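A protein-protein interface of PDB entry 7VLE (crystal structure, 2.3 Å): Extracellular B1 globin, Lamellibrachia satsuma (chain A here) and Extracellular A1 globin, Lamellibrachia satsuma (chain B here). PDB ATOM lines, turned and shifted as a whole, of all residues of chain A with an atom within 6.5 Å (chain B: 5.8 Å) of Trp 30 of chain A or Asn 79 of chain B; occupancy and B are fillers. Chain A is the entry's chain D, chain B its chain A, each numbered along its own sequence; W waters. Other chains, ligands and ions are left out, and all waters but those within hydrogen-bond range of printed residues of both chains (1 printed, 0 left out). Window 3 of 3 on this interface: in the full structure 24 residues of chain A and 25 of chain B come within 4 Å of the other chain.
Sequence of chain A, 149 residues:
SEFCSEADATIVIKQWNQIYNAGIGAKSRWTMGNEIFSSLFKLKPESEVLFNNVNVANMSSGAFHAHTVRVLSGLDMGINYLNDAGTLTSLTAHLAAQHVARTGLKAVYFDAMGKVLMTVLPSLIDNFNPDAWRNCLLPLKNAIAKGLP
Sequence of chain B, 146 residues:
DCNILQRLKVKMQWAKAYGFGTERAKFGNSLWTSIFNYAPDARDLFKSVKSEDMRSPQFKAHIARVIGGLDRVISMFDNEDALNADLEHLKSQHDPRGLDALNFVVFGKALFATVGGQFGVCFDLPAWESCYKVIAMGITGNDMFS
Of the 19 printed residues of chain A, 5 touch a printed residue of chain B.
Among the printed residues, 6 pairs touch across the chains.
Water W1 bridges a ring nitrogen (ND1) of His 65 of chain A (2.9 Å) and the side-chain amide oxygen of Asn 79 of chain B (3.0 Å).
The side-chain amide oxygen (OD1) of Asn 79 of chain B lies close to the backbone NH (N) of Asp 81 of chain B, at 3.4 Å.
The backbone NH of Ala 82 of chain B is in hydrogen-bond range of the side-chain amide oxygen of Asn 79 of chain B.
The indole nitrogen (NE1) of Trp 30 of chain A lies close to the backbone carbonyl oxygen (O) of Lys 27 of chain A, at 3.4 Å.
ND2 of Asn 34 of chain A lies close to O of Trp 30 of chain A (3.3 Å).
Among the printed residues, pairs that only touch across the chains: Ala 26 of chain A with Met 76 of chain B (3.7 Å), Trp 30 of chain A with Asn 79 of chain B (3.3 Å), Gly 62 of chain A with Asp 81 of chain B (3.7 Å), Gly 62 of chain A with Ala 82 of chain B (3.5 Å), Ala 66 of chain A with Ala 82 of chain B (3.7 Å) and Val 69 of chain A with Met 76 of chain B (3.8 Å).
Of chain B, only Asn 79 (3.3 Å) comes within 4 Å of Trp 30 of chain A.
Asn 79 of chain B touches just one residue of chain A: Trp 30 (3.3 Å).
Of the printed residues of chain B, Ala 66 of chain A touches Ala 82.
Printed residues of chain B within 4 Å of Val 69 of chain A: Met 76.
Of the printed residues of chain B, Gly 62 of chain A touches Asp 81 (3.7 Å) and Ala 82 (3.5 Å).
Of the printed residues of chain A, Ala 82 of chain B touches Gly 62 (3.5 Å) and Ala 66 (3.7 Å).
Of the printed residues of chain A, Asp 81 of chain B touches Gly 62 (3.7 Å).
Gly 25 of chain A touches none of the printed residues of chain B.
Leu 83 of chain B touches none of the printed residues of chain A.
The nearest residue of chain B that does not touch Trp 30 of chain A is Ala 82 of chain B (4.1 Å).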
ATOM      1  N   GLY A  25      26.433  24.829  37.287  1.00  0.00           N
ATOM      2  CA  GLY A  25      25.955  26.036  36.640  1.00  0.00           C
ATOM      3  C   GLY A  25      26.744  26.363  35.385  1.00  0.00           C
ATOM      4  O   GLY A  25      27.949  26.119  35.294  1.00  0.00           O
ATOM      5  N   ALA A  26      26.041  26.946  34.410  1.00  0.00           N
ATOM      6  CA  ALA A  26      26.616  27.184  33.090  1.00  0.00           C
ATOM      7  C   ALA A  26      27.798  28.144  33.121  1.00  0.00           C
ATOM      8  O   ALA A  26      28.566  28.186  32.153  1.00  0.00           O
ATOM      9  CB  ALA A  26      25.543  27.721  32.142  1.00  0.00           C
ATOM     10  N   LYS A  27      27.960  28.916  34.199  1.00  0.00           N
ATOM     11  CA  LYS A  27      29.083  29.848  34.276  1.00  0.00           C
ATOM     12  C   LYS A  27      30.414  29.108  34.282  1.00  0.00           C
ATOM     13  O   LYS A  27      31.367  29.521  33.610  1.00  0.00           O
ATOM     14  CB  LYS A  27      28.960  30.725  35.521  1.00  0.00           C
ATOM     15  CG  LYS A  27      30.055  31.775  35.623  1.00  0.00           C
ATOM     16  CD  LYS A  27      30.176  32.348  37.025  1.00  0.00           C
ATOM     17  CE  LYS A  27      29.030  33.286  37.360  1.00  0.00           C
ATOM     18  NZ  LYS A  27      29.186  33.860  38.726  1.00  0.00           N
ATOM     19  N   SER A  28      30.504  28.021  35.046  1.00  0.00           N
ATOM     20  CA  SER A  28      31.706  27.199  35.011  1.00  0.00           C
ATOM     21  C   SER A  28      31.811  26.436  33.700  1.00  0.00           C
ATOM     22  O   SER A  28      32.916  26.070  33.281  1.00  0.00           O
ATOM     23  CB  SER A  28      31.696  26.227  36.179  1.00  0.00           C
ATOM     24  OG  SER A  28      30.602  25.363  36.021  1.00  0.00           O
ATOM     25  N   ARG A  29      30.672  26.186  33.048  1.00  0.00           N
ATOM     26  CA  ARG A  29      30.674  25.502  31.759  1.00  0.00           C
ATOM     27  C   ARG A  29      31.399  26.324  30.702  1.00  0.00           C
ATOM     28  O   ARG A  29      32.289  25.818  30.011  1.00  0.00           O
ATOM     29  CB  ARG A  29      29.237  25.208  31.321  1.00  0.00           C
ATOM     30  CG  ARG A  29      28.709  23.841  31.731  1.00  0.00           C
ATOM     31  CD  ARG A  29      27.225  23.719  31.407  1.00  0.00           C
ATOM     32  NE  ARG A  29      26.811  22.340  31.158  1.00  0.00           N
ATOM     33  CZ  ARG A  29      26.286  21.535  32.075  1.00  0.00           C
ATOM     34  NH1 ARG A  29      26.107  21.963  33.318  1.00  0.00           N
ATOM     35  NH2 ARG A  29      25.936  20.298  31.749  1.00  0.00           N
ATOM     36  N   TRP A  30      31.034  27.601  30.557  1.00  0.00           N
ATOM     37  CA  TRP A  30      31.681  28.418  29.538  1.00  0.00           C
ATOM     38  C   TRP A  30      33.023  28.977  29.997  1.00  0.00           C
ATOM     39  O   TRP A  30      33.824  29.387  29.151  1.00  0.00           O
ATOM     40  CB  TRP A  30      30.758  29.554  29.079  1.00  0.00           C
ATOM     41  CG  TRP A  30      30.395  30.582  30.116  1.00  0.00           C
ATOM     42  CD1 TRP A  30      31.248  31.398  30.803  1.00  0.00           C
ATOM     43  CD2 TRP A  30      29.073  30.939  30.543  1.00  0.00           C
ATOM     44  NE1 TRP A  30      30.542  32.220  31.648  1.00  0.00           N
ATOM     45  CE2 TRP A  30      29.204  31.960  31.505  1.00  0.00           C
ATOM     46  CE3 TRP A  30      27.792  30.486  30.211  1.00  0.00           C
ATOM     47  CZ2 TRP A  30      28.105  32.534  32.139  1.00  0.00           C
ATOM     48  CZ3 TRP A  30      26.701  31.058  30.843  1.00  0.00           C
ATOM     49  CH2 TRP A  30      26.866  32.070  31.796  1.00  0.00           C
ATOM     50  N   THR A  31      33.283  29.010  31.308  1.00  0.00           N
ATOM     51  CA  THR A  31      34.630  29.312  31.783  1.00  0.00           C
ATOM     52  C   THR A  31      35.622  28.285  31.259  1.00  0.00           C
ATOM     53  O   THR A  31      36.671  28.636  30.706  1.00  0.00           O
ATOM     54  CB  THR A  31      34.668  29.339  33.311  1.00  0.00           C
ATOM     55  OG1 THR A  31      33.777  30.347  33.804  1.00  0.00           O
ATOM     56  CG2 THR A  31      36.081  29.629  33.799  1.00  0.00           C
ATOM     57  N   MET A  32      35.304  27.001  31.440  1.00  0.00           N
ATOM     58  CA  MET A  32      36.104  25.942  30.840  1.00  0.00           C
ATOM     59  C   MET A  32      36.123  26.066  29.325  1.00  0.00           C
ATOM     60  O   MET A  32      37.176  25.917  28.695  1.00  0.00           O
ATOM     61  CB  MET A  32      35.557  24.577  31.256  1.00  0.00           C
ATOM     62  CG  MET A  32      35.715  24.256  32.730  1.00  0.00           C
ATOM     63  SD  MET A  32      34.899  22.708  33.167  1.00  0.00           S
ATOM     64  CE  MET A  32      35.484  21.640  31.855  1.00  0.00           C
ATOM     65  N   GLY A  33      34.965  26.346  28.721  1.00  0.00           N
ATOM     66  CA  GLY A  33      34.908  26.488  27.277  1.00  0.00           C
ATOM     67  C   GLY A  33      35.742  27.648  26.769  1.00  0.00           C
ATOM     68  O   GLY A  33      36.419  27.535  25.744  1.00  0.00           O
ATOM     69  N   ASN A  34      35.706  28.780  27.479  1.00  0.00           N
ATOM     70  CA  ASN A  34      36.516  29.927  27.080  1.00  0.00           C
ATOM     71  C   ASN A  34      38.004  29.622  27.199  1.00  0.00           C
ATOM     72  O   ASN A  34      38.788  29.990  26.317  1.00  0.00           O
ATOM     73  CB  ASN A  34      36.155  31.152  27.922  1.00  0.00           C
ATOM     74  CG  ASN A  34      34.934  31.881  27.398  1.00  0.00           C
ATOM     75  OD1 ASN A  34      34.660  31.876  26.197  1.00  0.00           O
ATOM     76  ND2 ASN A  34      34.195  32.520  28.298  1.00  0.00           N
ATOM     77  N   GLU A  35      38.410  28.959  28.284  1.00  0.00           N
ATOM     78  CA  GLU A  35      39.812  28.583  28.444  1.00  0.00           C
ATOM     79  C   GLU A  35      40.255  27.624  27.346  1.00  0.00           C
ATOM     80  O   GLU A  35      41.367  27.742  26.819  1.00  0.00           O
ATOM     81  CB  GLU A  35      40.033  27.955  29.821  1.00  0.00           C
ATOM     82  CG  GLU A  35      39.885  28.925  30.977  1.00  0.00           C
ATOM     83  CD  GLU A  35      40.921  30.030  30.938  1.00  0.00           C
ATOM     84  OE1 GLU A  35      42.127  29.712  30.866  1.00  0.00           O
ATOM     85  OE2 GLU A  35      40.528  31.214  30.967  1.00  0.00           O
ATOM     86  N   MET A  59      33.930  36.833  23.238  1.00  0.00           N
ATOM     87  CA  MET A  59      33.785  35.542  23.896  1.00  0.00           C
ATOM     88  C   MET A  59      33.002  35.628  25.200  1.00  0.00           C
ATOM     89  O   MET A  59      32.835  34.607  25.874  1.00  0.00           O
ATOM     90  CB  MET A  59      35.165  34.930  24.138  1.00  0.00           C
ATOM     91  CG  MET A  59      35.950  34.716  22.850  1.00  0.00           C
ATOM     92  SD  MET A  59      37.619  34.086  23.094  1.00  0.00           S
ATOM     93  CE  MET A  59      37.277  32.519  23.889  1.00  0.00           C
ATOM     94  N   GLY A  62      26.409  36.029  24.576  1.00  0.00           N
ATOM     95  CA  GLY A  62      25.511  34.901  24.753  1.00  0.00           C
ATOM     96  C   GLY A  62      25.634  33.875  23.647  1.00  0.00           C
ATOM     97  O   GLY A  62      25.429  32.679  23.877  1.00  0.00           O
ATOM     98  N   PHE A  64      28.450  33.015  21.865  1.00  0.00           N
ATOM     99  CA  PHE A  64      29.652  32.193  21.953  1.00  0.00           C
ATOM    100  C   PHE A  64      29.653  31.322  23.201  1.00  0.00           C
ATOM    101  O   PHE A  64      30.151  30.190  23.164  1.00  0.00           O
ATOM    102  CB  PHE A  64      30.904  33.068  21.923  1.00  0.00           C
ATOM    103  CG  PHE A  64      32.175  32.282  21.794  1.00  0.00           C
ATOM    104  CD1 PHE A  64      32.558  31.766  20.568  1.00  0.00           C
ATOM    105  CD2 PHE A  64      32.978  32.043  22.897  1.00  0.00           C
ATOM    106  CE1 PHE A  64      33.721  31.034  20.440  1.00  0.00           C
ATOM    107  CE2 PHE A  64      34.145  31.312  22.776  1.00  0.00           C
ATOM    108  CZ  PHE A  64      34.517  30.807  21.545  1.00  0.00           C
ATOM    109  N   HIS A  65      29.134  31.840  24.317  1.00  0.00           N
ATOM    110  CA  HIS A  65      28.902  30.999  25.487  1.00  0.00           C
ATOM    111  C   HIS A  65      28.092  29.770  25.103  1.00  0.00           C
ATOM    112  O   HIS A  65      28.424  28.641  25.483  1.00  0.00           O
ATOM    113  CB  HIS A  65      28.175  31.792  26.576  1.00  0.00           C
ATOM    114  CG  HIS A  65      29.070  32.658  27.405  1.00  0.00           C
ATOM    115  ND1 HIS A  65      28.582  33.563  28.325  1.00  0.00           N
ATOM    116  CD2 HIS A  65      30.419  32.754  27.465  1.00  0.00           C
ATOM    117  CE1 HIS A  65      29.591  34.181  28.910  1.00  0.00           C
ATOM    118  NE2 HIS A  65      30.718  33.709  28.406  1.00  0.00           N
ATOM    119  N   ALA A  66      27.029  29.981  24.322  1.00  0.00           N
ATOM    120  CA  ALA A  66      26.177  28.880  23.890  1.00  0.00           C
ATOM    121  C   ALA A  66      26.931  27.906  22.996  1.00  0.00           C
ATOM    122  O   ALA A  66      26.706  26.692  23.066  1.00  0.00           O
ATOM    123  CB  ALA A  66      24.948  29.429  23.167  1.00  0.00           C
ATOM    124  N   THR A  68      30.280  27.175  23.009  1.00  0.00           N
ATOM    125  CA  THR A  68      31.147  26.362  23.856  1.00  0.00           C
ATOM    126  C   THR A  68      30.337  25.379  24.687  1.00  0.00           C
ATOM    127  O   THR A  68      30.775  24.246  24.924  1.00  0.00           O
ATOM    128  CB  THR A  68      31.986  27.258  24.766  1.00  0.00           C
ATOM    129  OG1 THR A  68      31.126  27.923  25.701  1.00  0.00           O
ATOM    130  CG2 THR A  68      32.735  28.298  23.951  1.00  0.00           C
ATOM    131  N   VAL A  69      29.151  25.795  25.138  1.00  0.00           N
ATOM    132  CA  VAL A  69      28.301  24.912  25.931  1.00  0.00           C
ATOM    133  C   VAL A  69      27.897  23.687  25.123  1.00  0.00           C
ATOM    134  O   VAL A  69      27.928  22.557  25.626  1.00  0.00           O
ATOM    135  CB  VAL A  69      27.070  25.678  26.451  1.00  0.00           C
ATOM    136  CG1 VAL A  69      25.973  24.708  26.861  1.00  0.00           C
ATOM    137  CG2 VAL A  69      27.453  26.564  27.627  1.00  0.00           C
ATOM    138  N   LEU A  72      31.084  21.372  24.568  1.00  0.00           N
ATOM    139  CA  LEU A  72      31.360  20.561  25.749  1.00  0.00           C
ATOM    140  C   LEU A  72      30.259  19.540  25.992  1.00  0.00           C
ATOM    141  O   LEU A  72      30.533  18.432  26.468  1.00  0.00           O
ATOM    142  CB  LEU A  72      31.526  21.465  26.968  1.00  0.00           C
ATOM    143  CG  LEU A  72      32.682  22.462  26.903  1.00  0.00           C
ATOM    144  CD1 LEU A  72      32.610  23.426  28.066  1.00  0.00           C
ATOM    145  CD2 LEU A  72      34.011  21.731  26.899  1.00  0.00           C
ATOM    146  N   MET B  76      21.787  26.217  31.324  1.00  0.00           N
ATOM    147  CA  MET B  76      21.856  27.646  31.052  1.00  0.00           C
ATOM    148  C   MET B  76      20.609  28.392  31.509  1.00  0.00           C
ATOM    149  O   MET B  76      20.419  29.551  31.126  1.00  0.00           O
ATOM    150  CB  MET B  76      22.087  27.886  29.557  1.00  0.00           C
ATOM    151  CG  MET B  76      23.468  27.475  29.069  1.00  0.00           C
ATOM    152  SD  MET B  76      23.691  27.735  27.298  1.00  0.00           S
ATOM    153  CE  MET B  76      22.620  26.465  26.637  1.00  0.00           C
ATOM    154  N   PHE B  77      19.766  27.753  32.327  1.00  0.00           N
ATOM    155  CA  PHE B  77      18.523  28.373  32.778  1.00  0.00           C
ATOM    156  C   PHE B  77      18.767  29.680  33.520  1.00  0.00           C
ATOM    157  O   PHE B  77      17.900  30.560  33.524  1.00  0.00           O
ATOM    158  CB  PHE B  77      17.755  27.404  33.680  1.00  0.00           C
ATOM    159  CG  PHE B  77      16.550  26.788  33.029  1.00  0.00           C
ATOM    160  CD1 PHE B  77      16.013  27.329  31.872  1.00  0.00           C
ATOM    161  CD2 PHE B  77      15.945  25.672  33.583  1.00  0.00           C
ATOM    162  CE1 PHE B  77      14.900  26.765  31.277  1.00  0.00           C
ATOM    163  CE2 PHE B  77      14.832  25.103  32.992  1.00  0.00           C
ATOM    164  CZ  PHE B  77      14.309  25.650  31.839  1.00  0.00           C
ATOM    165  N   ASP B  78      19.927  29.826  34.153  1.00  0.00           N
ATOM    166  CA  ASP B  78      20.223  31.000  34.963  1.00  0.00           C
ATOM    167  C   ASP B  78      20.959  32.092  34.193  1.00  0.00           C
ATOM    168  O   ASP B  78      21.347  33.098  34.797  1.00  0.00           O
ATOM    169  CB  ASP B  78      21.029  30.593  36.200  1.00  0.00           C
ATOM    170  CG  ASP B  78      22.097  29.561  35.890  1.00  0.00           C
ATOM    171  OD1 ASP B  78      22.250  29.200  34.705  1.00  0.00           O
ATOM    172  OD2 ASP B  78      22.781  29.110  36.834  1.00  0.00           O
ATOM    173  N   ASN B  79      21.155  31.931  32.884  1.00  0.00           N
ATOM    174  CA  ASN B  79      21.795  32.957  32.058  1.00  0.00           C
ATOM    175  C   ASN B  79      20.972  33.168  30.790  1.00  0.00           C
ATOM    176  O   ASN B  79      21.089  32.398  29.832  1.00  0.00           O
ATOM    177  CB  ASN B  79      23.234  32.585  31.723  1.00  0.00           C
ATOM    178  CG  ASN B  79      23.967  33.709  31.020  1.00  0.00           C
ATOM    179  OD1 ASN B  79      23.887  33.851  29.801  1.00  0.00           O
ATOM    180  ND2 ASN B  79      24.675  34.528  31.792  1.00  0.00           N
ATOM    181  N   GLU B  80      20.169  34.237  30.789  1.00  0.00           N
ATOM    182  CA  GLU B  80      19.259  34.519  29.680  1.00  0.00           C
ATOM    183  C   GLU B  80      19.990  34.602  28.342  1.00  0.00           C
ATOM    184  O   GLU B  80      19.514  34.061  27.336  1.00  0.00           O
ATOM    185  CB  GLU B  80      18.511  35.825  29.953  1.00  0.00           C
ATOM    186  CG  GLU B  80      17.367  35.695  30.938  1.00  0.00           C
ATOM    187  CD  GLU B  80      16.102  35.183  30.284  1.00  0.00           C
ATOM    188  OE1 GLU B  80      15.605  35.848  29.350  1.00  0.00           O
ATOM    189  OE2 GLU B  80      15.608  34.111  30.693  1.00  0.00           O
ATOM    190  N   ASP B  81      21.138  35.285  28.313  1.00  0.00           N
ATOM    191  CA  ASP B  81      21.861  35.503  27.059  1.00  0.00           C
ATOM    192  C   ASP B  81      22.247  34.185  26.400  1.00  0.00           C
ATOM    193  O   ASP B  81      21.962  33.961  25.218  1.00  0.00           O
ATOM    194  CB  ASP B  81      23.112  36.344  27.314  1.00  0.00           C
ATOM    195  CG  ASP B  81      22.793  37.782  27.648  1.00  0.00           C
ATOM    196  OD1 ASP B  81      21.701  38.254  27.272  1.00  0.00           O
ATOM    197  OD2 ASP B  81      23.643  38.445  28.282  1.00  0.00           O
ATOM    198  N   ALA B  82      22.928  33.313  27.143  1.00  0.00           N
ATOM    199  CA  ALA B  82      23.335  32.027  26.589  1.00  0.00           C
ATOM    200  C   ALA B  82      22.125  31.150  26.297  1.00  0.00           C
ATOM    201  O   ALA B  82      22.104  30.421  25.299  1.00  0.00           O
ATOM    202  CB  ALA B  82      24.292  31.323  27.550  1.00  0.00           C
ATOM    203  N   LEU B  83      21.108  31.222  27.156  1.00  0.00           N
ATOM    204  CA  LEU B  83      19.911  30.404  26.995  1.00  0.00           C
ATOM    205  C   LEU B  83      19.204  30.706  25.680  1.00  0.00           C
ATOM    206  O   LEU B  83      18.992  29.813  24.852  1.00  0.00           O
ATOM    207  CB  LEU B  83      18.967  30.639  28.174  1.00  0.00           C
ATOM    208  CG  LEU B  83      17.643  29.883  28.116  1.00  0.00           C
ATOM    209  CD1 LEU B  83      17.894  28.394  28.267  1.00  0.00           C
ATOM    210  CD2 LEU B  83      16.676  30.388  29.178  1.00  0.00           C
ATOM    211  N   ASN B  84      18.821  31.970  25.481  1.00  0.00           N
ATOM    212  CA  ASN B  84      18.084  32.344  24.278  1.00  0.00           C
ATOM    213  C   ASN B  84      18.909  32.089  23.024  1.00  0.00           C
ATOM    214  O   ASN B  84      18.371  31.663  21.996  1.00  0.00           O
ATOM    215  CB  ASN B  84      17.665  33.811  24.358  1.00  0.00           C
ATOM    216  CG  ASN B  84      16.697  34.076  25.492  1.00  0.00           C
ATOM    217  OD1 ASN B  84      15.832  33.253  25.788  1.00  0.00           O
ATOM    218  ND2 ASN B  84      16.839  35.229  26.136  1.00  0.00           N
HETATM  219  O   HOH W   1      26.039  34.895  27.960  1.00  0.00           O
